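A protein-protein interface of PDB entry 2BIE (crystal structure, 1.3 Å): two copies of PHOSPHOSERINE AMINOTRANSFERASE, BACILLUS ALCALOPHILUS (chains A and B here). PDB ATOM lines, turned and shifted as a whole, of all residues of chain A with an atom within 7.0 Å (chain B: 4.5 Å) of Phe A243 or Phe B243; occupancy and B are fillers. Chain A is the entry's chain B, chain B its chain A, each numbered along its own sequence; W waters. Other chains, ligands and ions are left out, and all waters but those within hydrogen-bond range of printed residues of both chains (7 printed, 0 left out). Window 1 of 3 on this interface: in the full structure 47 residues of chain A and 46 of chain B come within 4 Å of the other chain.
The backbone carbonyl oxygen (O) of Pro A240 lies within hydrogen-bond range of the side-chain hydroxyl (OG) of Ser B202 (3.2 Å).
OG of Ser B202 lies within hydrogen-bond range of N of Thr A242, at 3.0 Å.
The side-chain hydroxyl (OG1) of Thr B242 sits at hydrogen-bond distance from the side-chain hydroxyl (OG) of Ser A202 (3.4 Å).
The side-chain hydroxyl (OG) of Ser B244 sits at hydrogen-bond distance from the backbone carbonyl oxygen (O) of Ser B202 (2.8 Å).
N of Met A38 lies close to OG of Ser A36, at 3.2 Å.
O of Ser A202 sits at hydrogen-bond distance from OG of Ser A244.
Among the printed residues, pairs that only touch across the chains: Leu A20 with Leu B27, Leu A20 with Met B38, Gln A24 with Leu B27, Met A38 with Phe B243, Met A38 with Met B247, Pro A201 with Met B38, Ser A202 with Pro B241, Pro A241 with Ser B202, Phe A243 with Met B38 and Phe A243 with Phe B243.
Of the printed residues of chain B, Leu A20 touches Leu B27 (3.8 Å) and Met B38 (3.7 Å).
Ala A23 touches none of the printed residues of chain B.
Printed residues of chain B within 4 Å of Pro A201: Met B38 (3.8 Å).
Of the printed residues of chain B, Pro A241 touches Ser B202 (3.6 Å).
Phe A243 touches two residues of chain B.
Of the printed residues of chain A, Leu B27 touches Leu A20 (3.8 Å) and Gln A24 (3.5 Å).
Of the printed residues of chain A, Pro B241 touches Ser A202.
Phe B243 touches just these residues of chain A: Met A38 (3.9 Å) and Phe A243 (3.4 Å).
Tyr B246 touches none of the printed residues of chain A.
The nearest printed residue of chain B that does not touch Pro A241 is Ser B244 (6.1 Å).
Hydrophobic or aromatic side chains of chain A that line the printed part of chain B: Leu A20, Met A38, Pro A201 and Phe A243.
Of the 11 printed residues of chain B, 7 touch a printed residue of chain A.
Along chain B the printed residues that touch a printed residue of chain A span positions 27 to 247.
Met A38 touches Phe B243, and with the chains exchanged Phe A243 touches Met B38.
Met A38 touches Met B247, but with the chains exchanged Met A247 does not touch Met B38 (4.03 Å).
Ser A202 touches Thr B242, and with the chains exchanged Thr A242 touches Ser B202.
Phe B243 touches its own counterpart, Phe A243.
Positions printed for both chains: 27, 37, 38, 202, 241, 242, 243, 244, 245, 246 and 247.
Water W2 lies within hydrogen-bond range of the side-chain hydroxyl of Ser B202 (2.7 Å), the side-chain hydroxyl of Thr A242 (3.2 Å) and the backbone NH of Phe A243 (3.2 Å).
Water W7 lies within hydrogen-bond range of O of Met A38 (2.7 Å), N of Ser B202 (3.1 Å) and OG1 of Thr A242 (3.5 Å).
Water W4 lies within hydrogen-bond range of the backbone carbonyl oxygen of Ser A202 (2.8 Å), the backbone NH of Phe B243 (3.0 Å) and the side-chain hydroxyl of Thr B242 (3.2 Å).
Water W6 lies within hydrogen-bond range of the backbone carbonyl oxygen of Met B38 (2.8 Å), the backbone NH of Ser A202 (2.9 Å) and the side-chain hydroxyl of Thr B242 (3.1 Å).
Water W3 bridges the side-chain hydroxyl (OG) of Ser A244 and the side-chain hydroxyl (OG) of Ser B244.
Water W1 lies within hydrogen-bond range of N of Ser B244 (3.0 Å), O of Ser A202 (3.1 Å), N of Phe B243 (3.4 Å) and O of Pro B241 (3.4 Å).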
ATOM      1  N   LEU A  20     -18.849  19.685   3.820  1.00  0.00           N
ATOM      2  CA  LEU A  20     -19.926  18.804   4.199  1.00  0.00           C
ATOM      3  C   LEU A  20     -19.865  17.476   3.443  1.00  0.00           C
ATOM      4  O   LEU A  20     -20.108  16.434   4.051  1.00  0.00           O
ATOM      5  CB  LEU A  20     -21.283  19.470   3.964  1.00  0.00           C
ATOM      6  CG  LEU A  20     -21.689  20.397   5.124  1.00  0.00           C
ATOM      7  CD1 LEU A  20     -22.826  21.335   4.716  1.00  0.00           C
ATOM      8  CD2 LEU A  20     -22.084  19.616   6.378  1.00  0.00           C
ATOM      9  N   ALA A  23     -17.214  15.442   5.061  1.00  0.00           N
ATOM     10  CA  ALA A  23     -17.682  14.932   6.318  1.00  0.00           C
ATOM     11  C   ALA A  23     -18.635  13.758   6.152  1.00  0.00           C
ATOM     12  O   ALA A  23     -18.550  12.753   6.855  1.00  0.00           O
ATOM     13  CB  ALA A  23     -18.351  16.031   7.128  1.00  0.00           C
ATOM     14  N   GLN A  24     -19.511  13.884   5.140  1.00  0.00           N
ATOM     15  CA  GLN A  24     -20.435  12.792   4.881  1.00  0.00           C
ATOM     16  C   GLN A  24     -19.703  11.543   4.489  1.00  0.00           C
ATOM     17  O   GLN A  24     -19.981  10.435   4.967  1.00  0.00           O
ATOM     18  CB  GLN A  24     -21.443  13.242   3.781  1.00  0.00           C
ATOM     19  CG  GLN A  24     -22.491  12.214   3.441  1.00  0.00           C
ATOM     20  CD  GLN A  24     -23.362  12.589   2.256  1.00  0.00           C
ATOM     21  OE1 GLN A  24     -22.772  12.962   1.224  1.00  0.00           O
ATOM     22  NE2 GLN A  24     -24.670  12.459   2.427  1.00  0.00           N
ATOM     23  N   LEU A  27     -17.997   9.854   7.466  1.00  0.00           N
ATOM     24  CA  LEU A  27     -18.662   9.939   8.776  1.00  0.00           C
ATOM     25  C   LEU A  27     -18.567   8.643   9.558  1.00  0.00           C
ATOM     26  O   LEU A  27     -18.604   8.697  10.789  1.00  0.00           O
ATOM     27  CB  LEU A  27     -20.139  10.364   8.558  1.00  0.00           C
ATOM     28  CG  LEU A  27     -20.783  10.990   9.793  1.00  0.00           C
ATOM     29  CD1 LEU A  27     -20.235  12.387   9.976  1.00  0.00           C
ATOM     30  CD2 LEU A  27     -22.302  11.024   9.705  1.00  0.00           C
ATOM     31  N   SER A  36     -16.165   6.743  13.430  1.00  0.00           N
ATOM     32  CA  SER A  36     -16.443   8.141  13.128  1.00  0.00           C
ATOM     33  C   SER A  36     -15.500   9.010  13.914  1.00  0.00           C
ATOM     34  O   SER A  36     -15.080   8.636  15.049  1.00  0.00           O
ATOM     35  CB  SER A  36     -17.878   8.453  13.565  1.00  0.00           C
ATOM     36  OG  SER A  36     -18.206   9.800  13.245  1.00  0.00           O
ATOM     37  N   VAL A  37     -15.217  10.197  13.412  1.00  0.00           N
ATOM     38  CA  VAL A  37     -14.487  11.168  14.225  1.00  0.00           C
ATOM     39  C   VAL A  37     -15.225  11.374  15.552  1.00  0.00           C
ATOM     40  O   VAL A  37     -14.616  11.649  16.615  1.00  0.00           O
ATOM     41  CB  VAL A  37     -14.274  12.450  13.363  1.00  0.00           C
ATOM     42  CG1 VAL A  37     -15.532  13.256  13.222  1.00  0.00           C
ATOM     43  CG2 VAL A  37     -13.177  13.309  13.988  1.00  0.00           C
ATOM     44  N   MET A  38     -16.556  11.238  15.597  1.00  0.00           N
ATOM     45  CA  MET A  38     -17.376  11.325  16.788  1.00  0.00           C
ATOM     46  C   MET A  38     -17.226  10.226  17.827  1.00  0.00           C
ATOM     47  O   MET A  38     -17.749  10.337  18.916  1.00  0.00           O
ATOM     48  CB  MET A  38     -18.921  11.287  16.401  1.00  0.00           C
ATOM     49  CG  MET A  38     -19.368  12.617  15.855  1.00  0.00           C
ATOM     50  SD  MET A  38     -21.137  12.520  15.462  1.00  0.00           S
ATOM     51  CE  MET A  38     -21.041  12.289  13.727  1.00  0.00           C
ATOM     52  N   TYR A  47      -7.672  11.977  17.090  1.00  0.00           N
ATOM     53  CA  TYR A  47      -8.363  13.255  17.306  1.00  0.00           C
ATOM     54  C   TYR A  47      -7.311  14.354  17.456  1.00  0.00           C
ATOM     55  O   TYR A  47      -7.500  15.476  16.969  1.00  0.00           O
ATOM     56  CB  TYR A  47      -9.347  13.184  18.536  1.00  0.00           C
ATOM     57  CG  TYR A  47      -9.803  14.631  18.683  1.00  0.00           C
ATOM     58  CD1 TYR A  47     -10.656  15.158  17.721  1.00  0.00           C
ATOM     59  CD2 TYR A  47      -9.348  15.410  19.727  1.00  0.00           C
ATOM     60  CE1 TYR A  47     -11.058  16.493  17.859  1.00  0.00           C
ATOM     61  CE2 TYR A  47      -9.717  16.713  19.813  1.00  0.00           C
ATOM     62  CZ  TYR A  47     -10.574  17.258  18.893  1.00  0.00           C
ATOM     63  OH  TYR A  47     -10.964  18.577  18.960  1.00  0.00           O
ATOM     64  N   PRO A 201     -19.753  24.811  12.178  1.00  0.00           N
ATOM     65  CA  PRO A 201     -21.047  24.683  12.823  1.00  0.00           C
ATOM     66  C   PRO A 201     -20.984  25.225  14.239  1.00  0.00           C
ATOM     67  O   PRO A 201     -19.916  25.544  14.791  1.00  0.00           O
ATOM     68  CB  PRO A 201     -21.276  23.170  12.870  1.00  0.00           C
ATOM     69  CG  PRO A 201     -19.880  22.655  13.134  1.00  0.00           C
ATOM     70  CD  PRO A 201     -18.998  23.562  12.269  1.00  0.00           C
ATOM     71  N   SER A 202     -22.162  25.387  14.829  1.00  0.00           N
ATOM     72  CA  SER A 202     -22.226  25.851  16.201  1.00  0.00           C
ATOM     73  C   SER A 202     -21.725  24.785  17.157  1.00  0.00           C
ATOM     74  O   SER A 202     -21.851  23.599  16.903  1.00  0.00           O
ATOM     75  CB  SER A 202     -23.630  26.313  16.611  1.00  0.00           C
ATOM     76  OG  SER A 202     -24.512  25.246  16.538  1.00  0.00           O
ATOM     77  N   VAL A 204     -18.541  25.278  18.872  1.00  0.00           N
ATOM     78  CA  VAL A 204     -17.192  25.688  19.240  1.00  0.00           C
ATOM     79  C   VAL A 204     -17.040  27.190  19.027  1.00  0.00           C
ATOM     80  O   VAL A 204     -17.612  27.761  18.111  1.00  0.00           O
ATOM     81  CB  VAL A 204     -16.133  24.865  18.517  1.00  0.00           C
ATOM     82  CG1 VAL A 204     -16.145  25.126  17.019  1.00  0.00           C
ATOM     83  CG2 VAL A 204     -14.739  25.081  19.141  1.00  0.00           C
ATOM     84  N   PRO A 240     -13.326  18.359  24.408  1.00  0.00           N
ATOM     85  CA  PRO A 240     -13.718  19.429  23.472  1.00  0.00           C
ATOM     86  C   PRO A 240     -14.887  18.940  22.640  1.00  0.00           C
ATOM     87  O   PRO A 240     -15.228  17.762  22.622  1.00  0.00           O
ATOM     88  CB  PRO A 240     -12.459  19.637  22.664  1.00  0.00           C
ATOM     89  CG  PRO A 240     -11.772  18.313  22.695  1.00  0.00           C
ATOM     90  CD  PRO A 240     -12.126  17.625  23.979  1.00  0.00           C
ATOM     91  N   PRO A 241     -15.497  19.884  21.920  1.00  0.00           N
ATOM     92  CA  PRO A 241     -16.529  19.569  20.915  1.00  0.00           C
ATOM     93  C   PRO A 241     -15.860  19.023  19.665  1.00  0.00           C
ATOM     94  O   PRO A 241     -15.558  19.740  18.702  1.00  0.00           O
ATOM     95  CB  PRO A 241     -17.214  20.917  20.721  1.00  0.00           C
ATOM     96  CG  PRO A 241     -16.126  21.926  20.928  1.00  0.00           C
ATOM     97  CD  PRO A 241     -15.298  21.343  22.086  1.00  0.00           C
ATOM     98  N   THR A 242     -15.548  17.732  19.737  1.00  0.00           N
ATOM     99  CA  THR A 242     -14.668  17.134  18.747  1.00  0.00           C
ATOM    100  C   THR A 242     -15.195  17.237  17.315  1.00  0.00           C
ATOM    101  O   THR A 242     -14.434  17.574  16.403  1.00  0.00           O
ATOM    102  CB  THR A 242     -14.318  15.671  19.080  1.00  0.00           C
ATOM    103  OG1 THR A 242     -15.553  14.954  19.219  1.00  0.00           O
ATOM    104  CG2 THR A 242     -13.510  15.542  20.372  1.00  0.00           C
ATOM    105  N   PHE A 243     -16.478  16.923  17.090  1.00  0.00           N
ATOM    106  CA  PHE A 243     -17.006  17.047  15.732  1.00  0.00           C
ATOM    107  C   PHE A 243     -17.028  18.483  15.240  1.00  0.00           C
ATOM    108  O   PHE A 243     -16.753  18.716  14.054  1.00  0.00           O
ATOM    109  CB  PHE A 243     -18.385  16.396  15.629  1.00  0.00           C
ATOM    110  CG  PHE A 243     -18.842  16.271  14.170  1.00  0.00           C
ATOM    111  CD1 PHE A 243     -18.299  15.307  13.335  1.00  0.00           C
ATOM    112  CD2 PHE A 243     -19.773  17.123  13.659  1.00  0.00           C
ATOM    113  CE1 PHE A 243     -18.689  15.200  12.024  1.00  0.00           C
ATOM    114  CE2 PHE A 243     -20.182  17.008  12.362  1.00  0.00           C
ATOM    115  CZ  PHE A 243     -19.627  16.059  11.547  1.00  0.00           C
ATOM    116  N   SER A 244     -17.356  19.416  16.112  1.00  0.00           N
ATOM    117  CA  SER A 244     -17.341  20.801  15.663  1.00  0.00           C
ATOM    118  C   SER A 244     -15.950  21.261  15.263  1.00  0.00           C
ATOM    119  O   SER A 244     -15.808  21.988  14.285  1.00  0.00           O
ATOM    120  CB  SER A 244     -17.904  21.706  16.754  1.00  0.00           C
ATOM    121  OG  SER A 244     -19.318  21.464  16.876  1.00  0.00           O
ATOM    122  N   ILE A 245     -14.917  20.816  16.019  1.00  0.00           N
ATOM    123  CA  ILE A 245     -13.559  21.197  15.643  1.00  0.00           C
ATOM    124  C   ILE A 245     -13.108  20.497  14.364  1.00  0.00           C
ATOM    125  O   ILE A 245     -12.408  21.072  13.520  1.00  0.00           O
ATOM    126  CB  ILE A 245     -12.634  20.914  16.828  1.00  0.00           C
ATOM    127  CG1 ILE A 245     -12.949  21.901  17.969  1.00  0.00           C
ATOM    128  CG2 ILE A 245     -11.164  20.961  16.455  1.00  0.00           C
ATOM    129  CD1 ILE A 245     -12.480  21.437  19.327  1.00  0.00           C
ATOM    130  N   TYR A 246     -13.487  19.234  14.162  1.00  0.00           N
ATOM    131  CA  TYR A 246     -13.286  18.538  12.888  1.00  0.00           C
ATOM    132  C   TYR A 246     -13.913  19.335  11.758  1.00  0.00           C
ATOM    133  O   TYR A 246     -13.325  19.526  10.702  1.00  0.00           O
ATOM    134  CB  TYR A 246     -13.837  17.111  13.014  1.00  0.00           C
ATOM    135  CG  TYR A 246     -14.092  16.475  11.671  1.00  0.00           C
ATOM    136  CD1 TYR A 246     -13.065  15.840  11.000  1.00  0.00           C
ATOM    137  CD2 TYR A 246     -15.360  16.497  11.100  1.00  0.00           C
ATOM    138  CE1 TYR A 246     -13.302  15.252   9.789  1.00  0.00           C
ATOM    139  CE2 TYR A 246     -15.563  15.917   9.865  1.00  0.00           C
ATOM    140  CZ  TYR A 246     -14.534  15.287   9.187  1.00  0.00           C
ATOM    141  OH  TYR A 246     -14.777  14.716   7.957  1.00  0.00           O
ATOM    142  N   MET A 247     -15.148  19.762  11.896  1.00  0.00           N
ATOM    143  CA  MET A 247     -15.820  20.498  10.832  1.00  0.00           C
ATOM    144  C   MET A 247     -15.121  21.836  10.576  1.00  0.00           C
ATOM    145  O   MET A 247     -14.997  22.253   9.437  1.00  0.00           O
ATOM    146  CB  MET A 247     -17.287  20.684  11.142  1.00  0.00           C
ATOM    147  CG  MET A 247     -18.177  19.512  11.009  1.00  0.00           C
ATOM    148  SD  MET A 247     -18.174  18.791   9.362  1.00  0.00           S
ATOM    149  CE  MET A 247     -18.527  20.209   8.337  1.00  0.00           C
ATOM    150  N   LEU A 248     -14.702  22.506  11.665  1.00  0.00           N
ATOM    151  CA  LEU A 248     -13.897  23.720  11.514  1.00  0.00           C
ATOM    152  C   LEU A 248     -12.684  23.460  10.662  1.00  0.00           C
ATOM    153  O   LEU A 248     -12.348  24.213   9.735  1.00  0.00           O
ATOM    154  CB  LEU A 248     -13.544  24.205  12.912  1.00  0.00           C
ATOM    155  CG  LEU A 248     -12.452  25.302  13.085  1.00  0.00           C
ATOM    156  CD1 LEU A 248     -12.936  26.577  12.509  1.00  0.00           C
ATOM    157  CD2 LEU A 248     -12.084  25.455  14.557  1.00  0.00           C
ATOM    158  N   ARG A 249     -11.975  22.363  10.960  1.00  0.00           N
ATOM    159  CA  ARG A 249     -10.806  21.997  10.161  1.00  0.00           C
ATOM    160  C   ARG A 249     -11.218  21.878   8.702  1.00  0.00           C
ATOM    161  O   ARG A 249     -10.527  22.400   7.791  1.00  0.00           O
ATOM    162  CB  ARG A 249     -10.201  20.694  10.714  1.00  0.00           C
ATOM    163  CG  ARG A 249      -8.889  20.280  10.121  1.00  0.00           C
ATOM    164  CD  ARG A 249      -8.851  19.647   8.764  1.00  0.00           C
ATOM    165  NE  ARG A 249      -9.770  18.531   8.559  1.00  0.00           N
ATOM    166  CZ  ARG A 249      -9.523  17.220   8.662  1.00  0.00           C
ATOM    167  NH1 ARG A 249      -8.339  16.700   8.978  1.00  0.00           N
ATOM    168  NH2 ARG A 249     -10.567  16.415   8.429  1.00  0.00           N
ATOM    169  N   LEU B  27     -27.024  14.161   5.863  1.00  0.00           N
ATOM    170  CA  LEU B  27     -26.086  15.210   6.266  1.00  0.00           C
ATOM    171  C   LEU B  27     -26.172  16.464   5.389  1.00  0.00           C
ATOM    172  O   LEU B  27     -25.892  17.571   5.873  1.00  0.00           O
ATOM    173  CB  LEU B  27     -24.629  14.715   6.275  1.00  0.00           C
ATOM    174  CG  LEU B  27     -23.725  15.546   7.168  1.00  0.00           C
ATOM    175  CD1 LEU B  27     -23.986  15.269   8.643  1.00  0.00           C
ATOM    176  CD2 LEU B  27     -22.273  15.250   6.888  1.00  0.00           C
ATOM    177  N   VAL B  37     -28.552  19.788   8.867  1.00  0.00           N
ATOM    178  CA  VAL B  37     -29.002  20.257  10.167  1.00  0.00           C
ATOM    179  C   VAL B  37     -28.020  21.289  10.693  1.00  0.00           C
ATOM    180  O   VAL B  37     -28.449  22.183  11.404  1.00  0.00           O
ATOM    181  CB  VAL B  37     -29.385  19.059  11.058  1.00  0.00           C
ATOM    182  CG1 VAL B  37     -28.104  18.399  11.508  1.00  0.00           C
ATOM    183  CG2 VAL B  37     -30.238  19.442  12.259  1.00  0.00           C
ATOM    184  N   MET B  38     -26.728  21.207  10.378  1.00  0.00           N
ATOM    185  CA  MET B  38     -25.666  22.104  10.794  1.00  0.00           C
ATOM    186  C   MET B  38     -25.762  23.472  10.154  1.00  0.00           C
ATOM    187  O   MET B  38     -25.053  24.402  10.581  1.00  0.00           O
ATOM    188  CB  MET B  38     -24.255  21.551  10.378  1.00  0.00           C
ATOM    189  CG  MET B  38     -23.637  20.595  11.361  1.00  0.00           C
ATOM    190  SD  MET B  38     -22.120  20.158  10.501  1.00  0.00           S
ATOM    191  CE  MET B  38     -22.579  18.600   9.869  1.00  0.00           C
ATOM    192  N   SER B 202     -20.015  14.586  21.718  1.00  0.00           N
ATOM    193  CA  SER B 202     -19.491  15.608  22.605  1.00  0.00           C
ATOM    194  C   SER B 202     -20.056  16.957  22.215  1.00  0.00           C
ATOM    195  O   SER B 202     -20.568  17.148  21.119  1.00  0.00           O
ATOM    196  CB  SER B 202     -17.945  15.672  22.566  1.00  0.00           C
ATOM    197  OG  SER B 202     -17.583  16.095  21.277  1.00  0.00           O
ATOM    198  N   PRO B 241     -25.658  23.882  20.515  1.00  0.00           N
ATOM    199  CA  PRO B 241     -24.854  22.947  19.709  1.00  0.00           C
ATOM    200  C   PRO B 241     -25.809  22.036  18.930  1.00  0.00           C
ATOM    201  O   PRO B 241     -26.158  20.940  19.333  1.00  0.00           O
ATOM    202  CB  PRO B 241     -24.064  22.211  20.749  1.00  0.00           C
ATOM    203  CG  PRO B 241     -24.959  22.173  21.952  1.00  0.00           C
ATOM    204  CD  PRO B 241     -25.644  23.515  21.937  1.00  0.00           C
ATOM    205  N   THR B 242     -26.227  22.570  17.770  1.00  0.00           N
ATOM    206  CA  THR B 242     -27.350  21.948  17.080  1.00  0.00           C
ATOM    207  C   THR B 242     -27.075  20.546  16.565  1.00  0.00           C
ATOM    208  O   THR B 242     -27.917  19.656  16.668  1.00  0.00           O
ATOM    209  CB  THR B 242     -27.847  22.826  15.906  1.00  0.00           C
ATOM    210  OG1 THR B 242     -26.728  23.129  15.094  1.00  0.00           O
ATOM    211  CG2 THR B 242     -28.466  24.132  16.388  1.00  0.00           C
ATOM    212  N   PHE B 243     -25.877  20.362  15.999  1.00  0.00           N
ATOM    213  CA  PHE B 243     -25.563  19.031  15.507  1.00  0.00           C
ATOM    214  C   PHE B 243     -25.406  18.052  16.669  1.00  0.00           C
ATOM    215  O   PHE B 243     -25.840  16.907  16.526  1.00  0.00           O
ATOM    216  CB  PHE B 243     -24.317  19.017  14.622  1.00  0.00           C
ATOM    217  CG  PHE B 243     -24.156  17.690  13.883  1.00  0.00           C
ATOM    218  CD1 PHE B 243     -24.994  17.357  12.849  1.00  0.00           C
ATOM    219  CD2 PHE B 243     -23.160  16.805  14.242  1.00  0.00           C
ATOM    220  CE1 PHE B 243     -24.877  16.161  12.169  1.00  0.00           C
ATOM    221  CE2 PHE B 243     -23.025  15.608  13.571  1.00  0.00           C
ATOM    222  CZ  PHE B 243     -23.870  15.305  12.534  1.00  0.00           C
ATOM    223  N   SER B 244     -24.827  18.478  17.769  1.00  0.00           N
ATOM    224  CA  SER B 244     -24.742  17.532  18.889  1.00  0.00           C
ATOM    225  C   SER B 244     -26.123  17.163  19.408  1.00  0.00           C
ATOM    226  O   SER B 244     -26.333  15.996  19.735  1.00  0.00           O
ATOM    227  CB  SER B 244     -23.931  18.147  20.034  1.00  0.00           C
ATOM    228  OG  SER B 244     -22.582  18.339  19.638  1.00  0.00           O
ATOM    229  N   ILE B 245     -27.048  18.136  19.471  1.00  0.00           N
ATOM    230  CA  ILE B 245     -28.387  17.794  19.967  1.00  0.00           C
ATOM    231  C   ILE B 245     -29.124  16.908  18.985  1.00  0.00           C
ATOM    232  O   ILE B 245     -29.858  15.974  19.368  1.00  0.00           O
ATOM    233  CB  ILE B 245     -29.119  19.104  20.308  1.00  0.00           C
ATOM    234  CG1 ILE B 245     -28.485  19.749  21.536  1.00  0.00           C
ATOM    235  CG2 ILE B 245     -30.592  18.856  20.487  1.00  0.00           C
ATOM    236  CD1 ILE B 245     -28.830  21.231  21.674  1.00  0.00           C
ATOM    237  N   TYR B 246     -28.937  17.139  17.678  1.00  0.00           N
ATOM    238  CA  TYR B 246     -29.435  16.258  16.648  1.00  0.00           C
ATOM    239  C   TYR B 246     -28.933  14.835  16.839  1.00  0.00           C
ATOM    240  O   TYR B 246     -29.666  13.838  16.765  1.00  0.00           O
ATOM    241  CB  TYR B 246     -29.057  16.848  15.274  1.00  0.00           C
ATOM    242  CG  TYR B 246     -29.193  15.859  14.151  1.00  0.00           C
ATOM    243  CD1 TYR B 246     -30.403  15.588  13.518  1.00  0.00           C
ATOM    244  CD2 TYR B 246     -28.071  15.143  13.717  1.00  0.00           C
ATOM    245  CE1 TYR B 246     -30.469  14.670  12.492  1.00  0.00           C
ATOM    246  CE2 TYR B 246     -28.177  14.223  12.722  1.00  0.00           C
ATOM    247  CZ  TYR B 246     -29.369  13.969  12.085  1.00  0.00           C
ATOM    248  OH  TYR B 246     -29.380  13.010  11.088  1.00  0.00           O
ATOM    249  N   MET B 247     -27.621  14.670  17.018  1.00  0.00           N
ATOM    250  CA  MET B 247     -27.073  13.334  17.207  1.00  0.00           C
ATOM    251  C   MET B 247     -27.607  12.688  18.463  1.00  0.00           C
ATOM    252  O   MET B 247     -27.883  11.475  18.461  1.00  0.00           O
ATOM    253  CB  MET B 247     -25.545  13.370  17.231  1.00  0.00           C
ATOM    254  CG  MET B 247     -24.857  13.613  15.917  1.00  0.00           C
ATOM    255  SD  MET B 247     -25.283  12.416  14.642  1.00  0.00           S
ATOM    256  CE  MET B 247     -24.842  10.903  15.444  1.00  0.00           C
HETATM  257  O   HOH W   1     -23.043  20.865  17.852  1.00  0.00           O
HETATM  258  O   HOH W   2     -18.654  15.491  18.907  1.00  0.00           O
HETATM  259  O   HOH W   3     -20.611  20.771  19.338  1.00  0.00           O
HETATM  260  O   HOH W   4     -23.681  22.312  15.239  1.00  0.00           O
HETATM  261  O   HOH W   5     -18.874  18.580  18.666  1.00  0.00           O
HETATM  262  O   HOH W   6     -24.494  24.454  13.360  1.00  0.00           O
HETATM  263  O   HOH W   7     -18.145  12.815  20.011  1.00  0.00           O
